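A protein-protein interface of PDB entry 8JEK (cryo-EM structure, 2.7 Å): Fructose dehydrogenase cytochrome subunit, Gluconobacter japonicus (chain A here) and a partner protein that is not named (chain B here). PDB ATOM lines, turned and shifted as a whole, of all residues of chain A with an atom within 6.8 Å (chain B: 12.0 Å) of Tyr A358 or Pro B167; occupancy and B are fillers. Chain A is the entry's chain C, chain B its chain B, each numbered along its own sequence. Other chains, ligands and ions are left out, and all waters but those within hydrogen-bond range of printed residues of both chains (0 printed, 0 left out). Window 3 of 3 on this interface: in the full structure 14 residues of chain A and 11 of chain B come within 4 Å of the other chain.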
ATOM      1  N   LYS A 257      -8.221 -20.517  -8.138  1.00  0.00           N
ATOM      2  CA  LYS A 257      -9.510 -20.718  -8.788  1.00  0.00           C
ATOM      3  C   LYS A 257     -10.593 -20.095  -7.925  1.00  0.00           C
ATOM      4  O   LYS A 257     -10.696 -20.401  -6.733  1.00  0.00           O
ATOM      5  CB  LYS A 257      -9.784 -22.207  -9.014  1.00  0.00           C
ATOM      6  CG  LYS A 257     -11.108 -22.508  -9.684  1.00  0.00           C
ATOM      7  CD  LYS A 257     -11.142 -23.939 -10.184  1.00  0.00           C
ATOM      8  CE  LYS A 257     -12.532 -24.338 -10.634  1.00  0.00           C
ATOM      9  NZ  LYS A 257     -12.528 -25.660 -11.317  1.00  0.00           N
ATOM     10  N   ARG A 262      -9.396 -16.267 -11.932  1.00  0.00           N
ATOM     11  CA  ARG A 262      -8.551 -17.428 -12.170  1.00  0.00           C
ATOM     12  C   ARG A 262      -7.127 -16.954 -12.417  1.00  0.00           C
ATOM     13  O   ARG A 262      -6.907 -16.019 -13.192  1.00  0.00           O
ATOM     14  CB  ARG A 262      -9.056 -18.249 -13.361  1.00  0.00           C
ATOM     15  CG  ARG A 262     -10.549 -18.518 -13.346  1.00  0.00           C
ATOM     16  CD  ARG A 262     -10.904 -19.643 -12.392  1.00  0.00           C
ATOM     17  NE  ARG A 262     -12.346 -19.799 -12.259  1.00  0.00           N
ATOM     18  CZ  ARG A 262     -13.024 -20.871 -12.645  1.00  0.00           C
ATOM     19  NH1 ARG A 262     -12.420 -21.913 -13.186  1.00  0.00           N
ATOM     20  NH2 ARG A 262     -14.344 -20.895 -12.487  1.00  0.00           N
ATOM     21  N   HIS A 347     -16.255 -21.450 -22.801  1.00  0.00           N
ATOM     22  CA  HIS A 347     -17.106 -20.386 -22.294  1.00  0.00           C
ATOM     23  C   HIS A 347     -18.350 -20.319 -23.160  1.00  0.00           C
ATOM     24  O   HIS A 347     -18.260 -20.289 -24.385  1.00  0.00           O
ATOM     25  CB  HIS A 347     -16.377 -19.044 -22.317  1.00  0.00           C
ATOM     26  CG  HIS A 347     -14.954 -19.120 -21.864  1.00  0.00           C
ATOM     27  ND1 HIS A 347     -14.596 -19.180 -20.535  1.00  0.00           N
ATOM     28  CD2 HIS A 347     -13.796 -19.138 -22.565  1.00  0.00           C
ATOM     29  CE1 HIS A 347     -13.282 -19.237 -20.437  1.00  0.00           C
ATOM     30  NE2 HIS A 347     -12.773 -19.212 -21.655  1.00  0.00           N
ATOM     31  N   SER A 354     -18.906 -22.684 -17.913  1.00  0.00           N
ATOM     32  CA  SER A 354     -19.497 -23.970 -17.588  1.00  0.00           C
ATOM     33  C   SER A 354     -20.246 -23.899 -16.259  1.00  0.00           C
ATOM     34  O   SER A 354     -20.044 -22.995 -15.445  1.00  0.00           O
ATOM     35  CB  SER A 354     -18.416 -25.046 -17.541  1.00  0.00           C
ATOM     36  OG  SER A 354     -18.722 -26.033 -16.580  1.00  0.00           O
ATOM     37  N   LYS A 355     -21.131 -24.873 -16.046  1.00  0.00           N
ATOM     38  CA  LYS A 355     -21.922 -24.927 -14.822  1.00  0.00           C
ATOM     39  C   LYS A 355     -21.118 -25.375 -13.613  1.00  0.00           C
ATOM     40  O   LYS A 355     -21.350 -24.876 -12.506  1.00  0.00           O
ATOM     41  CB  LYS A 355     -23.123 -25.859 -15.004  1.00  0.00           C
ATOM     42  CG  LYS A 355     -24.229 -25.285 -15.866  1.00  0.00           C
ATOM     43  CD  LYS A 355     -25.421 -26.224 -15.929  1.00  0.00           C
ATOM     44  CE  LYS A 355     -26.577 -25.597 -16.688  1.00  0.00           C
ATOM     45  NZ  LYS A 355     -26.248 -25.377 -18.121  1.00  0.00           N
ATOM     46  N   ASP A 356     -20.183 -26.303 -13.790  1.00  0.00           N
ATOM     47  CA  ASP A 356     -19.349 -26.778 -12.696  1.00  0.00           C
ATOM     48  C   ASP A 356     -18.138 -25.890 -12.448  1.00  0.00           C
ATOM     49  O   ASP A 356     -17.355 -26.174 -11.536  1.00  0.00           O
ATOM     50  CB  ASP A 356     -18.898 -28.220 -12.957  1.00  0.00           C
ATOM     51  CG  ASP A 356     -18.020 -28.351 -14.184  1.00  0.00           C
ATOM     52  OD1 ASP A 356     -17.991 -27.417 -15.007  1.00  0.00           O
ATOM     53  OD2 ASP A 356     -17.352 -29.395 -14.321  1.00  0.00           O
ATOM     54  N   GLY A 357     -17.965 -24.832 -13.234  1.00  0.00           N
ATOM     55  CA  GLY A 357     -16.913 -23.869 -13.006  1.00  0.00           C
ATOM     56  C   GLY A 357     -15.568 -24.202 -13.607  1.00  0.00           C
ATOM     57  O   GLY A 357     -14.629 -23.417 -13.431  1.00  0.00           O
ATOM     58  N   TYR A 358     -15.430 -25.332 -14.305  1.00  0.00           N
ATOM     59  CA  TYR A 358     -14.153 -25.641 -14.941  1.00  0.00           C
ATOM     60  C   TYR A 358     -13.794 -24.587 -15.978  1.00  0.00           C
ATOM     61  O   TYR A 358     -12.640 -24.152 -16.061  1.00  0.00           O
ATOM     62  CB  TYR A 358     -14.192 -27.029 -15.580  1.00  0.00           C
ATOM     63  CG  TYR A 358     -12.826 -27.534 -15.995  1.00  0.00           C
ATOM     64  CD1 TYR A 358     -12.281 -27.192 -17.224  1.00  0.00           C
ATOM     65  CD2 TYR A 358     -12.079 -28.340 -15.152  1.00  0.00           C
ATOM     66  CE1 TYR A 358     -11.035 -27.642 -17.601  1.00  0.00           C
ATOM     67  CE2 TYR A 358     -10.831 -28.795 -15.522  1.00  0.00           C
ATOM     68  CZ  TYR A 358     -10.315 -28.444 -16.749  1.00  0.00           C
ATOM     69  OH  TYR A 358      -9.072 -28.896 -17.124  1.00  0.00           O
ATOM     70  N   TYR A 359     -14.769 -24.164 -16.776  1.00  0.00           N
ATOM     71  CA  TYR A 359     -14.572 -23.073 -17.711  1.00  0.00           C
ATOM     72  C   TYR A 359     -15.151 -21.807 -17.107  1.00  0.00           C
ATOM     73  O   TYR A 359     -16.373 -21.727 -16.910  1.00  0.00           O
ATOM     74  CB  TYR A 359     -15.228 -23.388 -19.047  1.00  0.00           C
ATOM     75  CG  TYR A 359     -14.663 -24.641 -19.667  1.00  0.00           C
ATOM     76  CD1 TYR A 359     -13.320 -24.723 -19.991  1.00  0.00           C
ATOM     77  CD2 TYR A 359     -15.461 -25.751 -19.902  1.00  0.00           C
ATOM     78  CE1 TYR A 359     -12.790 -25.861 -20.542  1.00  0.00           C
ATOM     79  CE2 TYR A 359     -14.936 -26.897 -20.457  1.00  0.00           C
ATOM     80  CZ  TYR A 359     -13.599 -26.945 -20.775  1.00  0.00           C
ATOM     81  OH  TYR A 359     -13.057 -28.078 -21.327  1.00  0.00           O
ATOM     82  N   PRO A 360     -14.325 -20.817 -16.782  1.00  0.00           N
ATOM     83  CA  PRO A 360     -14.805 -19.688 -15.983  1.00  0.00           C
ATOM     84  C   PRO A 360     -15.808 -18.829 -16.732  1.00  0.00           C
ATOM     85  O   PRO A 360     -15.823 -18.766 -17.964  1.00  0.00           O
ATOM     86  CB  PRO A 360     -13.525 -18.900 -15.682  1.00  0.00           C
ATOM     87  CG  PRO A 360     -12.585 -19.287 -16.748  1.00  0.00           C
ATOM     88  CD  PRO A 360     -12.892 -20.706 -17.090  1.00  0.00           C
ATOM     89  N   HIS A 391      -3.398 -31.479 -10.257  1.00  0.00           N
ATOM     90  CA  HIS A 391      -4.450 -31.393 -11.261  1.00  0.00           C
ATOM     91  C   HIS A 391      -4.235 -30.126 -12.073  1.00  0.00           C
ATOM     92  O   HIS A 391      -4.010 -29.055 -11.502  1.00  0.00           O
ATOM     93  CB  HIS A 391      -5.839 -31.391 -10.617  1.00  0.00           C
ATOM     94  CG  HIS A 391      -6.953 -31.148 -11.586  1.00  0.00           C
ATOM     95  ND1 HIS A 391      -7.329 -32.074 -12.534  1.00  0.00           N
ATOM     96  CD2 HIS A 391      -7.774 -30.084 -11.752  1.00  0.00           C
ATOM     97  CE1 HIS A 391      -8.333 -31.592 -13.243  1.00  0.00           C
ATOM     98  NE2 HIS A 391      -8.622 -30.387 -12.789  1.00  0.00           N
ATOM     99  N   GLU A 392      -4.311 -30.244 -13.397  1.00  0.00           N
ATOM    100  CA  GLU A 392      -3.882 -29.184 -14.304  1.00  0.00           C
ATOM    101  C   GLU A 392      -5.070 -28.580 -15.050  1.00  0.00           C
ATOM    102  O   GLU A 392      -5.740 -29.269 -15.826  1.00  0.00           O
ATOM    103  CB  GLU A 392      -2.848 -29.720 -15.290  1.00  0.00           C
ATOM    104  CG  GLU A 392      -1.929 -28.657 -15.855  1.00  0.00           C
ATOM    105  CD  GLU A 392      -1.285 -29.073 -17.158  1.00  0.00           C
ATOM    106  OE1 GLU A 392      -0.567 -30.091 -17.171  1.00  0.00           O
ATOM    107  OE2 GLU A 392      -1.495 -28.379 -18.172  1.00  0.00           O
ATOM    108  N   ILE A 393      -5.332 -27.295 -14.793  1.00  0.00           N
ATOM    109  CA  ILE A 393      -5.995 -26.451 -15.779  1.00  0.00           C
ATOM    110  C   ILE A 393      -5.079 -26.230 -16.968  1.00  0.00           C
ATOM    111  O   ILE A 393      -3.883 -25.955 -16.809  1.00  0.00           O
ATOM    112  CB  ILE A 393      -6.396 -25.084 -15.188  1.00  0.00           C
ATOM    113  CG1 ILE A 393      -7.739 -25.093 -14.428  1.00  0.00           C
ATOM    114  CG2 ILE A 393      -6.252 -23.999 -16.243  1.00  0.00           C
ATOM    115  CD1 ILE A 393      -7.936 -26.257 -13.474  1.00  0.00           C
ATOM    116  N   LEU A 394      -5.654 -26.306 -18.168  1.00  0.00           N
ATOM    117  CA  LEU A 394      -5.009 -25.753 -19.349  1.00  0.00           C
ATOM    118  C   LEU A 394      -6.058 -25.157 -20.275  1.00  0.00           C
ATOM    119  O   LEU A 394      -6.984 -25.850 -20.704  1.00  0.00           O
ATOM    120  CB  LEU A 394      -4.190 -26.812 -20.092  1.00  0.00           C
ATOM    121  CG  LEU A 394      -3.241 -26.261 -21.157  1.00  0.00           C
ATOM    122  CD1 LEU A 394      -1.912 -26.985 -21.107  1.00  0.00           C
ATOM    123  CD2 LEU A 394      -3.854 -26.364 -22.537  1.00  0.00           C
ATOM    124  N   VAL B 158     -25.238 -33.767 -24.906  1.00  0.00           N
ATOM    125  CA  VAL B 158     -24.467 -32.616 -25.351  1.00  0.00           C
ATOM    126  C   VAL B 158     -24.974 -32.139 -26.706  1.00  0.00           C
ATOM    127  O   VAL B 158     -25.402 -32.937 -27.550  1.00  0.00           O
ATOM    128  CB  VAL B 158     -22.972 -32.983 -25.405  1.00  0.00           C
ATOM    129  CG1 VAL B 158     -22.714 -34.050 -26.455  1.00  0.00           C
ATOM    130  CG2 VAL B 158     -22.124 -31.765 -25.673  1.00  0.00           C
ATOM    131  N   PRO B 160     -23.245 -31.020 -29.713  1.00  0.00           N
ATOM    132  CA  PRO B 160     -21.832 -31.400 -29.864  1.00  0.00           C
ATOM    133  C   PRO B 160     -20.779 -30.302 -29.790  1.00  0.00           C
ATOM    134  O   PRO B 160     -19.924 -30.347 -28.903  1.00  0.00           O
ATOM    135  CB  PRO B 160     -21.831 -32.068 -31.240  1.00  0.00           C
ATOM    136  CG  PRO B 160     -23.137 -32.778 -31.254  1.00  0.00           C
ATOM    137  CD  PRO B 160     -24.115 -31.843 -30.571  1.00  0.00           C
ATOM    138  N   TYR B 162     -20.565 -27.611 -28.465  1.00  0.00           N
ATOM    139  CA  TYR B 162     -20.569 -26.849 -27.228  1.00  0.00           C
ATOM    140  C   TYR B 162     -20.482 -27.819 -26.060  1.00  0.00           C
ATOM    141  O   TYR B 162     -20.995 -28.938 -26.127  1.00  0.00           O
ATOM    142  CB  TYR B 162     -21.822 -25.980 -27.113  1.00  0.00           C
ATOM    143  CG  TYR B 162     -21.957 -24.981 -28.237  1.00  0.00           C
ATOM    144  CD1 TYR B 162     -22.591 -25.321 -29.423  1.00  0.00           C
ATOM    145  CD2 TYR B 162     -21.433 -23.702 -28.119  1.00  0.00           C
ATOM    146  CE1 TYR B 162     -22.709 -24.415 -30.452  1.00  0.00           C
ATOM    147  CE2 TYR B 162     -21.545 -22.790 -29.143  1.00  0.00           C
ATOM    148  CZ  TYR B 162     -22.185 -23.150 -30.308  1.00  0.00           C
ATOM    149  OH  TYR B 162     -22.298 -22.241 -31.332  1.00  0.00           O
ATOM    150  N   ALA B 163     -19.832 -27.387 -24.987  1.00  0.00           N
ATOM    151  CA  ALA B 163     -19.434 -28.280 -23.908  1.00  0.00           C
ATOM    152  C   ALA B 163     -20.465 -28.293 -22.789  1.00  0.00           C
ATOM    153  O   ALA B 163     -20.951 -27.237 -22.369  1.00  0.00           O
ATOM    154  CB  ALA B 163     -18.070 -27.872 -23.350  1.00  0.00           C
ATOM    155  N   HIS B 164     -20.802 -29.492 -22.320  1.00  0.00           N
ATOM    156  CA  HIS B 164     -21.400 -29.662 -21.007  1.00  0.00           C
ATOM    157  C   HIS B 164     -20.370 -29.322 -19.927  1.00  0.00           C
ATOM    158  O   HIS B 164     -19.189 -29.088 -20.203  1.00  0.00           O
ATOM    159  CB  HIS B 164     -21.900 -31.095 -20.835  1.00  0.00           C
ATOM    160  CG  HIS B 164     -23.390 -31.228 -20.779  1.00  0.00           C
ATOM    161  ND1 HIS B 164     -24.072 -31.448 -19.603  1.00  0.00           N
ATOM    162  CD2 HIS B 164     -24.326 -31.188 -21.754  1.00  0.00           C
ATOM    163  CE1 HIS B 164     -25.366 -31.534 -19.855  1.00  0.00           C
ATOM    164  NE2 HIS B 164     -25.546 -31.377 -21.153  1.00  0.00           N
ATOM    165  N   ASN B 165     -20.818 -29.319 -18.676  1.00  0.00           N
ATOM    166  CA  ASN B 165     -19.981 -28.787 -17.607  1.00  0.00           C
ATOM    167  C   ASN B 165     -18.817 -29.705 -17.243  1.00  0.00           C
ATOM    168  O   ASN B 165     -18.975 -30.633 -16.445  1.00  0.00           O
ATOM    169  CB  ASN B 165     -20.828 -28.499 -16.365  1.00  0.00           C
ATOM    170  CG  ASN B 165     -21.676 -29.677 -15.947  1.00  0.00           C
ATOM    171  OD1 ASN B 165     -21.741 -30.687 -16.643  1.00  0.00           O
ATOM    172  ND2 ASN B 165     -22.325 -29.555 -14.799  1.00  0.00           N
ATOM    173  N   GLY B 166     -17.639 -29.444 -17.807  1.00  0.00           N
ATOM    174  CA  GLY B 166     -16.424 -30.060 -17.329  1.00  0.00           C
ATOM    175  C   GLY B 166     -15.942 -31.242 -18.144  1.00  0.00           C
ATOM    176  O   GLY B 166     -16.719 -31.948 -18.791  1.00  0.00           O
ATOM    177  N   PRO B 167     -14.627 -31.483 -18.110  1.00  0.00           N
ATOM    178  CA  PRO B 167     -14.038 -32.550 -18.928  1.00  0.00           C
ATOM    179  C   PRO B 167     -14.371 -33.970 -18.490  1.00  0.00           C
ATOM    180  O   PRO B 167     -13.910 -34.908 -19.147  1.00  0.00           O
ATOM    181  CB  PRO B 167     -12.532 -32.288 -18.795  1.00  0.00           C
ATOM    182  CG  PRO B 167     -12.438 -30.843 -18.537  1.00  0.00           C
ATOM    183  CD  PRO B 167     -13.601 -30.542 -17.638  1.00  0.00           C
ATOM    184  N   ASN B 168     -15.112 -34.184 -17.402  1.00  0.00           N
ATOM    185  CA  ASN B 168     -15.474 -35.548 -17.029  1.00  0.00           C
ATOM    186  C   ASN B 168     -16.894 -35.628 -16.480  1.00  0.00           C
ATOM    187  O   ASN B 168     -17.178 -36.453 -15.606  1.00  0.00           O
ATOM    188  CB  ASN B 168     -14.487 -36.125 -16.014  1.00  0.00           C
ATOM    189  CG  ASN B 168     -13.384 -36.932 -16.667  1.00  0.00           C
ATOM    190  OD1 ASN B 168     -13.553 -37.460 -17.763  1.00  0.00           O
ATOM    191  ND2 ASN B 168     -12.246 -37.031 -15.995  1.00  0.00           N
ATOM    192  N   TYR B 169     -17.798 -34.784 -16.985  1.00  0.00           N
ATOM    193  CA  TYR B 169     -19.139 -34.681 -16.422  1.00  0.00           C
ATOM    194  C   TYR B 169     -19.942 -35.968 -16.552  1.00  0.00           C
ATOM    195  O   TYR B 169     -20.932 -36.139 -15.833  1.00  0.00           O
ATOM    196  CB  TYR B 169     -19.897 -33.534 -17.094  1.00  0.00           C
ATOM    197  CG  TYR B 169     -20.352 -33.839 -18.503  1.00  0.00           C
ATOM    198  CD1 TYR B 169     -19.519 -33.606 -19.587  1.00  0.00           C
ATOM    199  CD2 TYR B 169     -21.617 -34.358 -18.751  1.00  0.00           C
ATOM    200  CE1 TYR B 169     -19.929 -33.887 -20.872  1.00  0.00           C
ATOM    201  CE2 TYR B 169     -22.032 -34.643 -20.031  1.00  0.00           C
ATOM    202  CZ  TYR B 169     -21.186 -34.405 -21.088  1.00  0.00           C
ATOM    203  OH  TYR B 169     -21.600 -34.686 -22.369  1.00  0.00           O
ATOM    204  N   TRP B 170     -19.547 -36.874 -17.443  1.00  0.00           N
ATOM    205  CA  TRP B 170     -20.387 -38.009 -17.798  1.00  0.00           C
ATOM    206  C   TRP B 170     -20.297 -39.167 -16.813  1.00  0.00           C
ATOM    207  O   TRP B 170     -20.951 -40.192 -17.032  1.00  0.00           O
ATOM    208  CB  TRP B 170     -20.034 -38.502 -19.202  1.00  0.00           C
ATOM    209  CG  TRP B 170     -18.569 -38.683 -19.438  1.00  0.00           C
ATOM    210  CD1 TRP B 170     -17.815 -39.769 -19.113  1.00  0.00           C
ATOM    211  CD2 TRP B 170     -17.681 -37.748 -20.055  1.00  0.00           C
ATOM    212  NE1 TRP B 170     -16.512 -39.571 -19.490  1.00  0.00           N
ATOM    213  CE2 TRP B 170     -16.403 -38.336 -20.072  1.00  0.00           C
ATOM    214  CE3 TRP B 170     -17.841 -36.472 -20.596  1.00  0.00           C
ATOM    215  CZ2 TRP B 170     -15.297 -37.691 -20.604  1.00  0.00           C
ATOM    216  CZ3 TRP B 170     -16.742 -35.835 -21.123  1.00  0.00           C
ATOM    217  CH2 TRP B 170     -15.487 -36.446 -21.130  1.00  0.00           C
ATOM    218  N   VAL B 171     -19.517 -39.041 -15.742  1.00  0.00           N
ATOM    219  CA  VAL B 171     -19.386 -40.113 -14.760  1.00  0.00           C
ATOM    220  C   VAL B 171     -20.603 -40.121 -13.846  1.00  0.00           C
ATOM    221  O   VAL B 171     -20.755 -41.013 -13.003  1.00  0.00           O
ATOM    222  CB  VAL B 171     -18.088 -39.970 -13.946  1.00  0.00           C
ATOM    223  CG1 VAL B 171     -16.919 -39.726 -14.871  1.00  0.00           C
ATOM    224  CG2 VAL B 171     -18.218 -38.849 -12.935  1.00  0.00           C
ATOM    225  N   SER B 172     -21.472 -39.130 -14.002  1.00  0.00           N
ATOM    226  CA  SER B 172     -22.697 -39.043 -13.226  1.00  0.00           C
ATOM    227  C   SER B 172     -23.806 -39.862 -13.879  1.00  0.00           C
ATOM    228  O   SER B 172     -23.733 -40.242 -15.049  1.00  0.00           O
ATOM    229  CB  SER B 172     -23.128 -37.586 -13.075  1.00  0.00           C
ATOM    230  OG  SER B 172     -23.464 -37.023 -14.330  1.00  0.00           O
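N of Gly B166 lies within hydrogen-bond range of OD1 of Asp A356.
The backbone carbonyl oxygen (O) of Asn B165 lies close to the side-chain carboxylate (OD2) of Asp A356.
The backbone NH of Asp A356 lies within hydrogen-bond range of the side-chain hydroxyl of Ser A354 (3.2 Å).
The backbone NH of Ser A354 is in hydrogen-bond range of the backbone carbonyl oxygen of Tyr A359.
OD1 of Asp A356 lies close to N of Tyr A358, at 3.4 Å.
OG of Ser A354 touches CA of Asn B165, at 3.2 Å.
Ser A354 touches Gly B166.
Lys A355 touches Asn B165 (N to CB, 3.7 Å).
Pro B167 touches Tyr A358.
CG of Pro B167 touches OH of Tyr A359, 3.98 Å away.
His A347 touches none of the printed residues of chain B.
Of the printed residues of chain B, Ser A354 touches Asn B165 (3.2 Å) and Gly B166 (3.8 Å).
Of the printed residues of chain B, Lys A355 touches Asn B165 (3.7 Å).
No residue of chain B comes within 4 Å of Pro A360.
His A391 touches none of the printed residues of chain B.
No residue of chain B comes within 4 Å of Ile A393.
Printed residues of chain A within 4 Å of Asn B165: Ser A354 (3.2 Å), Lys A355 (3.7 Å) and Asp A356 (2.9 Å).
Of the printed residues of chain A, Gly B166 touches Ser A354 and Asp A356.
Pro B167 touches just these residues of chain A: Tyr A358 and Tyr A359.
Of the 13 printed residues of chain B, 3 touch a printed residue of chain A.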
